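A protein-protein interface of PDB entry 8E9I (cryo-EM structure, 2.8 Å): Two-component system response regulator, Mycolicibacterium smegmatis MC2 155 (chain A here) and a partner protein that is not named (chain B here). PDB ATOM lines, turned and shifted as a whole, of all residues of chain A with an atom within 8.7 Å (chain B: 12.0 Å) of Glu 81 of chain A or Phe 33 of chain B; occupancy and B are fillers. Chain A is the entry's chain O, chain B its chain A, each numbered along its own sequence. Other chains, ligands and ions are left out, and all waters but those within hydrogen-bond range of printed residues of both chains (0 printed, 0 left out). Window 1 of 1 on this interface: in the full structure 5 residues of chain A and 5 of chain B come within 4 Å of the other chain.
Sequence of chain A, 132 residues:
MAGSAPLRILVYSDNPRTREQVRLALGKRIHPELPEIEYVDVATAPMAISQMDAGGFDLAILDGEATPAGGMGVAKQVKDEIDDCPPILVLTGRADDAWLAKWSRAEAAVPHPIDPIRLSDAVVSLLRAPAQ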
ATOM      1  N   ALA A  45      35.502 -10.153  -9.557  1.00  0.00           N
ATOM      2  CA  ALA A  45      34.373 -10.051 -10.468  1.00  0.00           C
ATOM      3  C   ALA A  45      34.558  -8.897 -11.446  1.00  0.00           C
ATOM      4  O   ALA A  45      34.328  -9.080 -12.644  1.00  0.00           O
ATOM      5  CB  ALA A  45      33.065  -9.891  -9.696  1.00  0.00           C
ATOM      6  N   ILE A  49      34.574  -9.492 -15.468  1.00  0.00           N
ATOM      7  CA  ILE A  49      33.604  -8.838 -16.335  1.00  0.00           C
ATOM      8  C   ILE A  49      34.319  -8.034 -17.412  1.00  0.00           C
ATOM      9  O   ILE A  49      33.949  -8.080 -18.587  1.00  0.00           O
ATOM     10  CB  ILE A  49      32.660  -7.954 -15.503  1.00  0.00           C
ATOM     11  CG1 ILE A  49      31.783  -8.812 -14.587  1.00  0.00           C
ATOM     12  CG2 ILE A  49      31.795  -7.102 -16.409  1.00  0.00           C
ATOM     13  CD1 ILE A  49      30.812  -9.716 -15.317  1.00  0.00           C
ATOM     14  N   SER A  50      35.350  -7.279 -17.028  1.00  0.00           N
ATOM     15  CA  SER A  50      36.054  -6.464 -18.012  1.00  0.00           C
ATOM     16  C   SER A  50      36.751  -7.322 -19.060  1.00  0.00           C
ATOM     17  O   SER A  50      36.733  -6.984 -20.247  1.00  0.00           O
ATOM     18  CB  SER A  50      37.060  -5.551 -17.316  1.00  0.00           C
ATOM     19  OG  SER A  50      38.181  -6.282 -16.859  1.00  0.00           O
ATOM     20  N   MET A  52      35.802 -10.326 -20.024  1.00  0.00           N
ATOM     21  CA  MET A  52      34.730 -10.788 -20.894  1.00  0.00           C
ATOM     22  C   MET A  52      34.322  -9.697 -21.873  1.00  0.00           C
ATOM     23  O   MET A  52      34.135  -9.960 -23.065  1.00  0.00           O
ATOM     24  CB  MET A  52      33.535 -11.220 -20.051  1.00  0.00           C
ATOM     25  CG  MET A  52      33.795 -12.434 -19.179  1.00  0.00           C
ATOM     26  SD  MET A  52      34.213 -13.895 -20.138  1.00  0.00           S
ATOM     27  CE  MET A  52      32.630 -14.209 -20.906  1.00  0.00           C
ATOM     28  N   ASP A  53      34.195  -8.464 -21.386  1.00  0.00           N
ATOM     29  CA  ASP A  53      33.836  -7.346 -22.248  1.00  0.00           C
ATOM     30  C   ASP A  53      34.868  -7.153 -23.350  1.00  0.00           C
ATOM     31  O   ASP A  53      34.529  -6.730 -24.461  1.00  0.00           O
ATOM     32  CB  ASP A  53      33.694  -6.075 -21.414  1.00  0.00           C
ATOM     33  N   GLY A  73      26.619 -15.942 -10.107  1.00  0.00           N
ATOM     34  CA  GLY A  73      26.170 -14.583 -10.345  1.00  0.00           C
ATOM     35  C   GLY A  73      26.893 -13.948 -11.513  1.00  0.00           C
ATOM     36  O   GLY A  73      26.279 -13.287 -12.355  1.00  0.00           O
ATOM     37  N   VAL A  74      28.205 -14.161 -11.599  1.00  0.00           N
ATOM     38  CA  VAL A  74      28.953 -13.633 -12.730  1.00  0.00           C
ATOM     39  C   VAL A  74      28.492 -14.291 -14.019  1.00  0.00           C
ATOM     40  O   VAL A  74      28.464 -13.656 -15.072  1.00  0.00           O
ATOM     41  CB  VAL A  74      30.464 -13.816 -12.517  1.00  0.00           C
ATOM     42  CG1 VAL A  74      31.222 -13.318 -13.726  1.00  0.00           C
ATOM     43  CG2 VAL A  74      30.918 -13.087 -11.276  1.00  0.00           C
ATOM     44  N   ALA A  75      28.133 -15.572 -13.965  1.00  0.00           N
ATOM     45  CA  ALA A  75      27.667 -16.254 -15.165  1.00  0.00           C
ATOM     46  C   ALA A  75      26.373 -15.633 -15.673  1.00  0.00           C
ATOM     47  O   ALA A  75      26.242 -15.308 -16.861  1.00  0.00           O
ATOM     48  CB  ALA A  75      27.475 -17.741 -14.876  1.00  0.00           C
ATOM     49  N   LYS A  76      25.405 -15.456 -14.779  1.00  0.00           N
ATOM     50  CA  LYS A  76      24.155 -14.830 -15.188  1.00  0.00           C
ATOM     51  C   LYS A  76      24.409 -13.427 -15.719  1.00  0.00           C
ATOM     52  O   LYS A  76      23.863 -13.036 -16.757  1.00  0.00           O
ATOM     53  CB  LYS A  76      23.177 -14.795 -14.016  1.00  0.00           C
ATOM     54  CG  LYS A  76      21.783 -14.312 -14.378  1.00  0.00           C
ATOM     55  CD  LYS A  76      21.128 -15.216 -15.409  1.00  0.00           C
ATOM     56  CE  LYS A  76      19.674 -14.855 -15.619  1.00  0.00           C
ATOM     57  NZ  LYS A  76      19.531 -13.596 -16.395  1.00  0.00           N
ATOM     58  N   GLN A  77      25.261 -12.666 -15.034  1.00  0.00           N
ATOM     59  CA  GLN A  77      25.577 -11.316 -15.480  1.00  0.00           C
ATOM     60  C   GLN A  77      26.176 -11.320 -16.881  1.00  0.00           C
ATOM     61  O   GLN A  77      25.734 -10.570 -17.757  1.00  0.00           O
ATOM     62  CB  GLN A  77      26.535 -10.660 -14.494  1.00  0.00           C
ATOM     63  CG  GLN A  77      26.955  -9.273 -14.884  1.00  0.00           C
ATOM     64  CD  GLN A  77      27.792  -8.615 -13.825  1.00  0.00           C
ATOM     65  OE1 GLN A  77      27.865  -9.094 -12.698  1.00  0.00           O
ATOM     66  NE2 GLN A  77      28.445  -7.519 -14.181  1.00  0.00           N
ATOM     67  N   VAL A  78      27.184 -12.160 -17.115  1.00  0.00           N
ATOM     68  CA  VAL A  78      27.871 -12.141 -18.401  1.00  0.00           C
ATOM     69  C   VAL A  78      26.923 -12.569 -19.509  1.00  0.00           C
ATOM     70  O   VAL A  78      27.003 -12.070 -20.636  1.00  0.00           O
ATOM     71  CB  VAL A  78      29.132 -13.024 -18.369  1.00  0.00           C
ATOM     72  CG1 VAL A  78      30.127 -12.489 -17.353  1.00  0.00           C
ATOM     73  CG2 VAL A  78      28.785 -14.464 -18.083  1.00  0.00           C
ATOM     74  N   LYS A  79      26.017 -13.499 -19.218  1.00  0.00           N
ATOM     75  CA  LYS A  79      25.051 -13.856 -20.248  1.00  0.00           C
ATOM     76  C   LYS A  79      24.043 -12.741 -20.480  1.00  0.00           C
ATOM     77  O   LYS A  79      23.498 -12.625 -21.582  1.00  0.00           O
ATOM     78  CB  LYS A  79      24.345 -15.159 -19.891  1.00  0.00           C
ATOM     79  CG  LYS A  79      25.163 -16.359 -20.284  1.00  0.00           C
ATOM     80  CD  LYS A  79      24.384 -17.642 -20.225  1.00  0.00           C
ATOM     81  CE  LYS A  79      25.156 -18.732 -20.928  1.00  0.00           C
ATOM     82  NZ  LYS A  79      25.149 -18.533 -22.399  1.00  0.00           N
ATOM     83  N   ASP A  80      23.783 -11.907 -19.473  1.00  0.00           N
ATOM     84  CA  ASP A  80      22.843 -10.813 -19.673  1.00  0.00           C
ATOM     85  C   ASP A  80      23.491  -9.576 -20.281  1.00  0.00           C
ATOM     86  O   ASP A  80      22.771  -8.700 -20.771  1.00  0.00           O
ATOM     87  CB  ASP A  80      22.183 -10.435 -18.345  1.00  0.00           C
ATOM     88  CG  ASP A  80      21.090 -11.402 -17.936  1.00  0.00           C
ATOM     89  OD1 ASP A  80      20.641 -12.198 -18.784  1.00  0.00           O
ATOM     90  OD2 ASP A  80      20.673 -11.365 -16.762  1.00  0.00           O
ATOM     91  N   GLU A  81      24.818  -9.485 -20.277  1.00  0.00           N
ATOM     92  CA  GLU A  81      25.498  -8.227 -20.555  1.00  0.00           C
ATOM     93  C   GLU A  81      26.421  -8.249 -21.762  1.00  0.00           C
ATOM     94  O   GLU A  81      26.660  -7.193 -22.345  1.00  0.00           O
ATOM     95  CB  GLU A  81      26.313  -7.790 -19.329  1.00  0.00           C
ATOM     96  CG  GLU A  81      25.461  -7.492 -18.116  1.00  0.00           C
ATOM     97  CD  GLU A  81      26.253  -6.889 -16.975  1.00  0.00           C
ATOM     98  OE1 GLU A  81      27.498  -6.850 -17.067  1.00  0.00           O
ATOM     99  OE2 GLU A  81      25.630  -6.471 -15.975  1.00  0.00           O
ATOM    100  N   ILE A  82      26.969  -9.398 -22.136  1.00  0.00           N
ATOM    101  CA  ILE A  82      27.844  -9.498 -23.300  1.00  0.00           C
ATOM    102  C   ILE A  82      27.065 -10.152 -24.431  1.00  0.00           C
ATOM    103  O   ILE A  82      26.610 -11.295 -24.304  1.00  0.00           O
ATOM    104  CB  ILE A  82      29.123 -10.290 -22.987  1.00  0.00           C
ATOM    105  CG1 ILE A  82      29.971  -9.561 -21.947  1.00  0.00           C
ATOM    106  CG2 ILE A  82      29.923 -10.519 -24.251  1.00  0.00           C
ATOM    107  CD1 ILE A  82      29.628  -9.914 -20.532  1.00  0.00           C
ATOM    108  N   ASP A  83      26.909  -9.431 -25.535  1.00  0.00           N
ATOM    109  CA  ASP A  83      26.352 -10.035 -26.735  1.00  0.00           C
ATOM    110  C   ASP A  83      27.351 -11.037 -27.293  1.00  0.00           C
ATOM    111  O   ASP A  83      28.564 -10.818 -27.229  1.00  0.00           O
ATOM    112  CB  ASP A  83      26.033  -8.962 -27.774  1.00  0.00           C
ATOM    113  N   ASP A  84      26.845 -12.140 -27.837  1.00  0.00           N
ATOM    114  CA  ASP A  84      27.701 -13.223 -28.315  1.00  0.00           C
ATOM    115  C   ASP A  84      28.654 -13.673 -27.209  1.00  0.00           C
ATOM    116  O   ASP A  84      29.869 -13.754 -27.395  1.00  0.00           O
ATOM    117  CB  ASP A  84      28.471 -12.800 -29.567  1.00  0.00           C
ATOM    118  N   CYS A  85      28.086 -13.941 -26.038  1.00  0.00           N
ATOM    119  CA  CYS A  85      28.889 -14.340 -24.895  1.00  0.00           C
ATOM    120  C   CYS A  85      29.392 -15.769 -25.090  1.00  0.00           C
ATOM    121  O   CYS A  85      28.656 -16.619 -25.604  1.00  0.00           O
ATOM    122  CB  CYS A  85      28.064 -14.237 -23.610  1.00  0.00           C
ATOM    123  SG  CYS A  85      28.978 -14.528 -22.081  1.00  0.00           S
ATOM    124  N   LEU B  26      20.704  10.715 -19.329  1.00  0.00           N
ATOM    125  CA  LEU B  26      21.145   9.695 -20.268  1.00  0.00           C
ATOM    126  C   LEU B  26      22.660   9.691 -20.429  1.00  0.00           C
ATOM    127  O   LEU B  26      23.247   8.653 -20.744  1.00  0.00           O
ATOM    128  CB  LEU B  26      20.469   9.905 -21.619  1.00  0.00           C
ATOM    129  CG  LEU B  26      18.950   9.748 -21.594  1.00  0.00           C
ATOM    130  CD1 LEU B  26      18.364  10.126 -22.942  1.00  0.00           C
ATOM    131  CD2 LEU B  26      18.550   8.336 -21.207  1.00  0.00           C
ATOM    132  N   GLY B  29      26.856   9.572 -15.558  1.00  0.00           N
ATOM    133  CA  GLY B  29      26.726   8.380 -14.762  1.00  0.00           C
ATOM    134  C   GLY B  29      27.056   7.135 -15.552  1.00  0.00           C
ATOM    135  O   GLY B  29      27.175   7.161 -16.780  1.00  0.00           O
ATOM    136  N   PRO B  30      27.200   6.010 -14.860  1.00  0.00           N
ATOM    137  CA  PRO B  30      27.544   4.766 -15.549  1.00  0.00           C
ATOM    138  C   PRO B  30      26.465   4.362 -16.537  1.00  0.00           C
ATOM    139  O   PRO B  30      25.300   4.744 -16.424  1.00  0.00           O
ATOM    140  CB  PRO B  30      27.660   3.746 -14.410  1.00  0.00           C
ATOM    141  CG  PRO B  30      27.850   4.557 -13.184  1.00  0.00           C
ATOM    142  CD  PRO B  30      27.077   5.810 -13.409  1.00  0.00           C
ATOM    143  N   ARG B  31      26.878   3.601 -17.539  1.00  0.00           N
ATOM    144  CA  ARG B  31      25.958   2.954 -18.456  1.00  0.00           C
ATOM    145  C   ARG B  31      26.520   1.598 -18.837  1.00  0.00           C
ATOM    146  O   ARG B  31      27.633   1.503 -19.358  1.00  0.00           O
ATOM    147  CB  ARG B  31      25.725   3.790 -19.710  1.00  0.00           C
ATOM    148  CG  ARG B  31      25.051   5.113 -19.445  1.00  0.00           C
ATOM    149  CD  ARG B  31      24.290   5.570 -20.666  1.00  0.00           C
ATOM    150  NE  ARG B  31      22.974   4.948 -20.735  1.00  0.00           N
ATOM    151  CZ  ARG B  31      22.623   4.015 -21.612  1.00  0.00           C
ATOM    152  NH1 ARG B  31      23.463   3.578 -22.539  1.00  0.00           N
ATOM    153  NH2 ARG B  31      21.397   3.505 -21.557  1.00  0.00           N
ATOM    154  N   ARG B  32      25.743   0.552 -18.578  1.00  0.00           N
ATOM    155  CA  ARG B  32      26.149  -0.802 -18.936  1.00  0.00           C
ATOM    156  C   ARG B  32      24.914  -1.563 -19.390  1.00  0.00           C
ATOM    157  O   ARG B  32      23.930  -1.652 -18.652  1.00  0.00           O
ATOM    158  CB  ARG B  32      26.823  -1.508 -17.768  1.00  0.00           C
ATOM    159  CG  ARG B  32      27.253  -2.911 -18.122  1.00  0.00           C
ATOM    160  CD  ARG B  32      28.152  -3.524 -17.084  1.00  0.00           C
ATOM    161  NE  ARG B  32      28.584  -4.849 -17.509  1.00  0.00           N
ATOM    162  CZ  ARG B  32      29.469  -5.068 -18.470  1.00  0.00           C
ATOM    163  NH1 ARG B  32      30.062  -4.070 -19.106  1.00  0.00           N
ATOM    164  NH2 ARG B  32      29.762  -6.319 -18.808  1.00  0.00           N
ATOM    165  N   PHE B  33      24.970  -2.112 -20.598  1.00  0.00           N
ATOM    166  CA  PHE B  33      23.851  -2.887 -21.103  1.00  0.00           C
ATOM    167  C   PHE B  33      23.683  -4.168 -20.298  1.00  0.00           C
ATOM    168  O   PHE B  33      24.654  -4.852 -19.971  1.00  0.00           O
ATOM    169  CB  PHE B  33      24.059  -3.218 -22.578  1.00  0.00           C
ATOM    170  CG  PHE B  33      23.087  -4.223 -23.107  1.00  0.00           C
ATOM    171  CD1 PHE B  33      21.839  -3.833 -23.545  1.00  0.00           C
ATOM    172  CD2 PHE B  33      23.422  -5.560 -23.161  1.00  0.00           C
ATOM    173  CE1 PHE B  33      20.942  -4.760 -24.028  1.00  0.00           C
ATOM    174  CE2 PHE B  33      22.533  -6.486 -23.643  1.00  0.00           C
ATOM    175  CZ  PHE B  33      21.290  -6.087 -24.075  1.00  0.00           C
ATOM    176  N   ASN B  34      22.436  -4.491 -19.979  1.00  0.00           N
ATOM    177  CA  ASN B  34      22.127  -5.747 -19.306  1.00  0.00           C
ATOM    178  C   ASN B  34      20.682  -6.088 -19.605  1.00  0.00           C
ATOM    179  O   ASN B  34      19.787  -5.300 -19.295  1.00  0.00           O
ATOM    180  CB  ASN B  34      22.353  -5.641 -17.807  1.00  0.00           C
ATOM    181  CG  ASN B  34      22.055  -6.936 -17.084  1.00  0.00           C
ATOM    182  OD1 ASN B  34      20.976  -7.505 -17.228  1.00  0.00           O
ATOM    183  ND2 ASN B  34      23.011  -7.404 -16.291  1.00  0.00           N
ATOM    184  N   ARG B  35      20.451  -7.256 -20.196  1.00  0.00           N
ATOM    185  CA  ARG B  35      19.093  -7.616 -20.573  1.00  0.00           C
ATOM    186  C   ARG B  35      18.183  -7.645 -19.353  1.00  0.00           C
ATOM    187  O   ARG B  35      17.036  -7.193 -19.415  1.00  0.00           O
ATOM    188  CB  ARG B  35      19.099  -8.964 -21.285  1.00  0.00           C
ATOM    189  CG  ARG B  35      19.815  -8.900 -22.615  1.00  0.00           C
ATOM    190  CD  ARG B  35      20.036 -10.269 -23.228  1.00  0.00           C
ATOM    191  NE  ARG B  35      20.586 -10.148 -24.572  1.00  0.00           N
ATOM    192  CZ  ARG B  35      21.851  -9.846 -24.831  1.00  0.00           C
ATOM    193  NH1 ARG B  35      22.736  -9.686 -23.864  1.00  0.00           N
ATOM    194  NH2 ARG B  35      22.240  -9.713 -26.095  1.00  0.00           N
ATOM    195  N   SER B  36      18.681  -8.168 -18.231  1.00  0.00           N
ATOM    196  CA  SER B  36      17.888  -8.187 -17.007  1.00  0.00           C
ATOM    197  C   SER B  36      17.579  -6.774 -16.531  1.00  0.00           C
ATOM    198  O   SER B  36      16.451  -6.475 -16.126  1.00  0.00           O
ATOM    199  CB  SER B  36      18.626  -8.970 -15.923  1.00  0.00           C
ATOM    200  OG  SER B  36      17.823  -9.123 -14.768  1.00  0.00           O
ATOM    201  N   LYS B  37      18.571  -5.887 -16.577  1.00  0.00           N
ATOM    202  CA  LYS B  37      18.346  -4.517 -16.134  1.00  0.00           C
ATOM    203  C   LYS B  37      17.290  -3.834 -16.983  1.00  0.00           C
ATOM    204  O   LYS B  37      16.459  -3.078 -16.470  1.00  0.00           O
ATOM    205  CB  LYS B  37      19.648  -3.728 -16.187  1.00  0.00           C
ATOM    206  CG  LYS B  37      19.531  -2.326 -15.639  1.00  0.00           C
ATOM    207  CD  LYS B  37      20.758  -1.495 -15.958  1.00  0.00           C
ATOM    208  CE  LYS B  37      21.983  -2.018 -15.238  1.00  0.00           C
ATOM    209  NZ  LYS B  37      23.200  -1.254 -15.604  1.00  0.00           N
ATOM    210  N   LEU B  38      17.316  -4.075 -18.288  1.00  0.00           N
ATOM    211  CA  LEU B  38      16.418  -3.405 -19.212  1.00  0.00           C
ATOM    212  C   LEU B  38      15.047  -4.059 -19.293  1.00  0.00           C
ATOM    213  O   LEU B  38      14.145  -3.493 -19.917  1.00  0.00           O
ATOM    214  CB  LEU B  38      17.048  -3.368 -20.604  1.00  0.00           C
ATOM    215  CG  LEU B  38      18.439  -2.739 -20.660  1.00  0.00           C
ATOM    216  CD1 LEU B  38      18.967  -2.778 -22.073  1.00  0.00           C
ATOM    217  CD2 LEU B  38      18.435  -1.319 -20.127  1.00  0.00           C
ATOM    218  N   GLU B  39      14.865  -5.226 -18.690  1.00  0.00           N
ATOM    219  CA  GLU B  39      13.564  -5.867 -18.696  1.00  0.00           C
ATOM    220  C   GLU B  39      12.609  -5.131 -17.761  1.00  0.00           C
ATOM    221  O   GLU B  39      13.016  -4.417 -16.842  1.00  0.00           O
ATOM    222  CB  GLU B  39      13.688  -7.335 -18.291  1.00  0.00           C
ATOM    223  N   ALA B  40      11.317  -5.315 -18.002  1.00  0.00           N
ATOM    224  CA  ALA B  40      10.312  -4.659 -17.182  1.00  0.00           C
ATOM    225  C   ALA B  40      10.470  -5.077 -15.730  1.00  0.00           C
ATOM    226  O   ALA B  40      10.898  -6.191 -15.424  1.00  0.00           O
ATOM    227  CB  ALA B  40       8.909  -5.011 -17.675  1.00  0.00           C
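OD2 of Asp 80 of chain A is in salt-bridge range of NZ of Lys 76 of chain A.
OD1 of Asn 34 of chain B sits at hydrogen-bond distance from N of Lys 37 of chain B.
O of Arg 32 of chain B is in hydrogen-bond range of NZ of Lys 37 of chain B (3.2 Å).
The side-chain carboxylate (OE1) of Glu 81 of chain A is in hydrogen-bond range of the side-chain amide nitrogen (NE2) of Gln 77 of chain A, 3.1 Å away.
N of Ser 36 of chain B lies within hydrogen-bond range of OD1 of Asn 34 of chain B (2.6 Å).
The side-chain carboxylate (OE2) of Glu 81 of chain A lies within hydrogen-bond range of the side-chain amide nitrogen (ND2) of Asn 34 of chain B, at 2.8 Å.
The side-chain carboxylate (OE1) of Glu 81 of chain A is in salt-bridge range of the guanidinium group (NH2) of Arg 32 of chain B (2.9 Å).
O of Asp 80 of chain A is in hydrogen-bond range of N of Arg 35 of chain B.
Glu 81 of chain A touches just these residues of chain B: Arg 32 (2.3 Å), Phe 33 (3.3 Å) and Asn 34 (2.8 Å).
Phe 33 of chain B touches just these residues of chain A: Asp 80 and Glu 81.
No residue of chain B comes within 4 Å of Val 78 of chain A.
Printed residues of chain B within 4 Å of Asp 80 of chain A: Phe 33, Asn 34, Arg 35 and Ser 36.
No residue of chain B comes within 4 Å of Asp 83 of chain A.
Of the printed residues of chain A, Arg 35 of chain B touches Lys 79 (3.8 Å) and Asp 80 (2.8 Å).
Of the printed residues of chain A, Arg 32 of chain B touches Ile 49 (3.2 Å), Glu 81 (2.3 Å) and Ile 82 (3.99 Å).
Of the printed residues of chain A, Ser 36 of chain B touches Asp 80 (3.3 Å).
Printed residues of chain B within 4 Å of Lys 79 of chain A: Arg 35 (3.8 Å).
Glu 39 of chain B touches none of the printed residues of chain A.
Lys 37 of chain B touches none of the printed residues of chain A.
The nearest residue of chain B that does not touch Glu 81 of chain A is Arg 35 of chain B (4.2 Å).
The nearest residue of chain A that does not touch Phe 33 of chain B is Ile 82 of chain A (5.3 Å).
Among the printed residues, pairs that only touch across the chains: Ile 49 of chain A with Arg 32 of chain B (3.2 Å), Lys 79 of chain A with Arg 35 of chain B (3.8 Å), Asp 80 of chain A with Phe 33 of chain B (3.6 Å), Asp 80 of chain A with Asn 34 of chain B (3.4 Å), Asp 80 of chain A with Ser 36 of chain B (3.3 Å), Glu 81 of chain A with Phe 33 of chain B (3.3 Å) and Ile 82 of chain A with Arg 32 of chain B (3.99 Å).
Of the 18 printed residues of chain A, 5 touch a printed residue of chain B.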
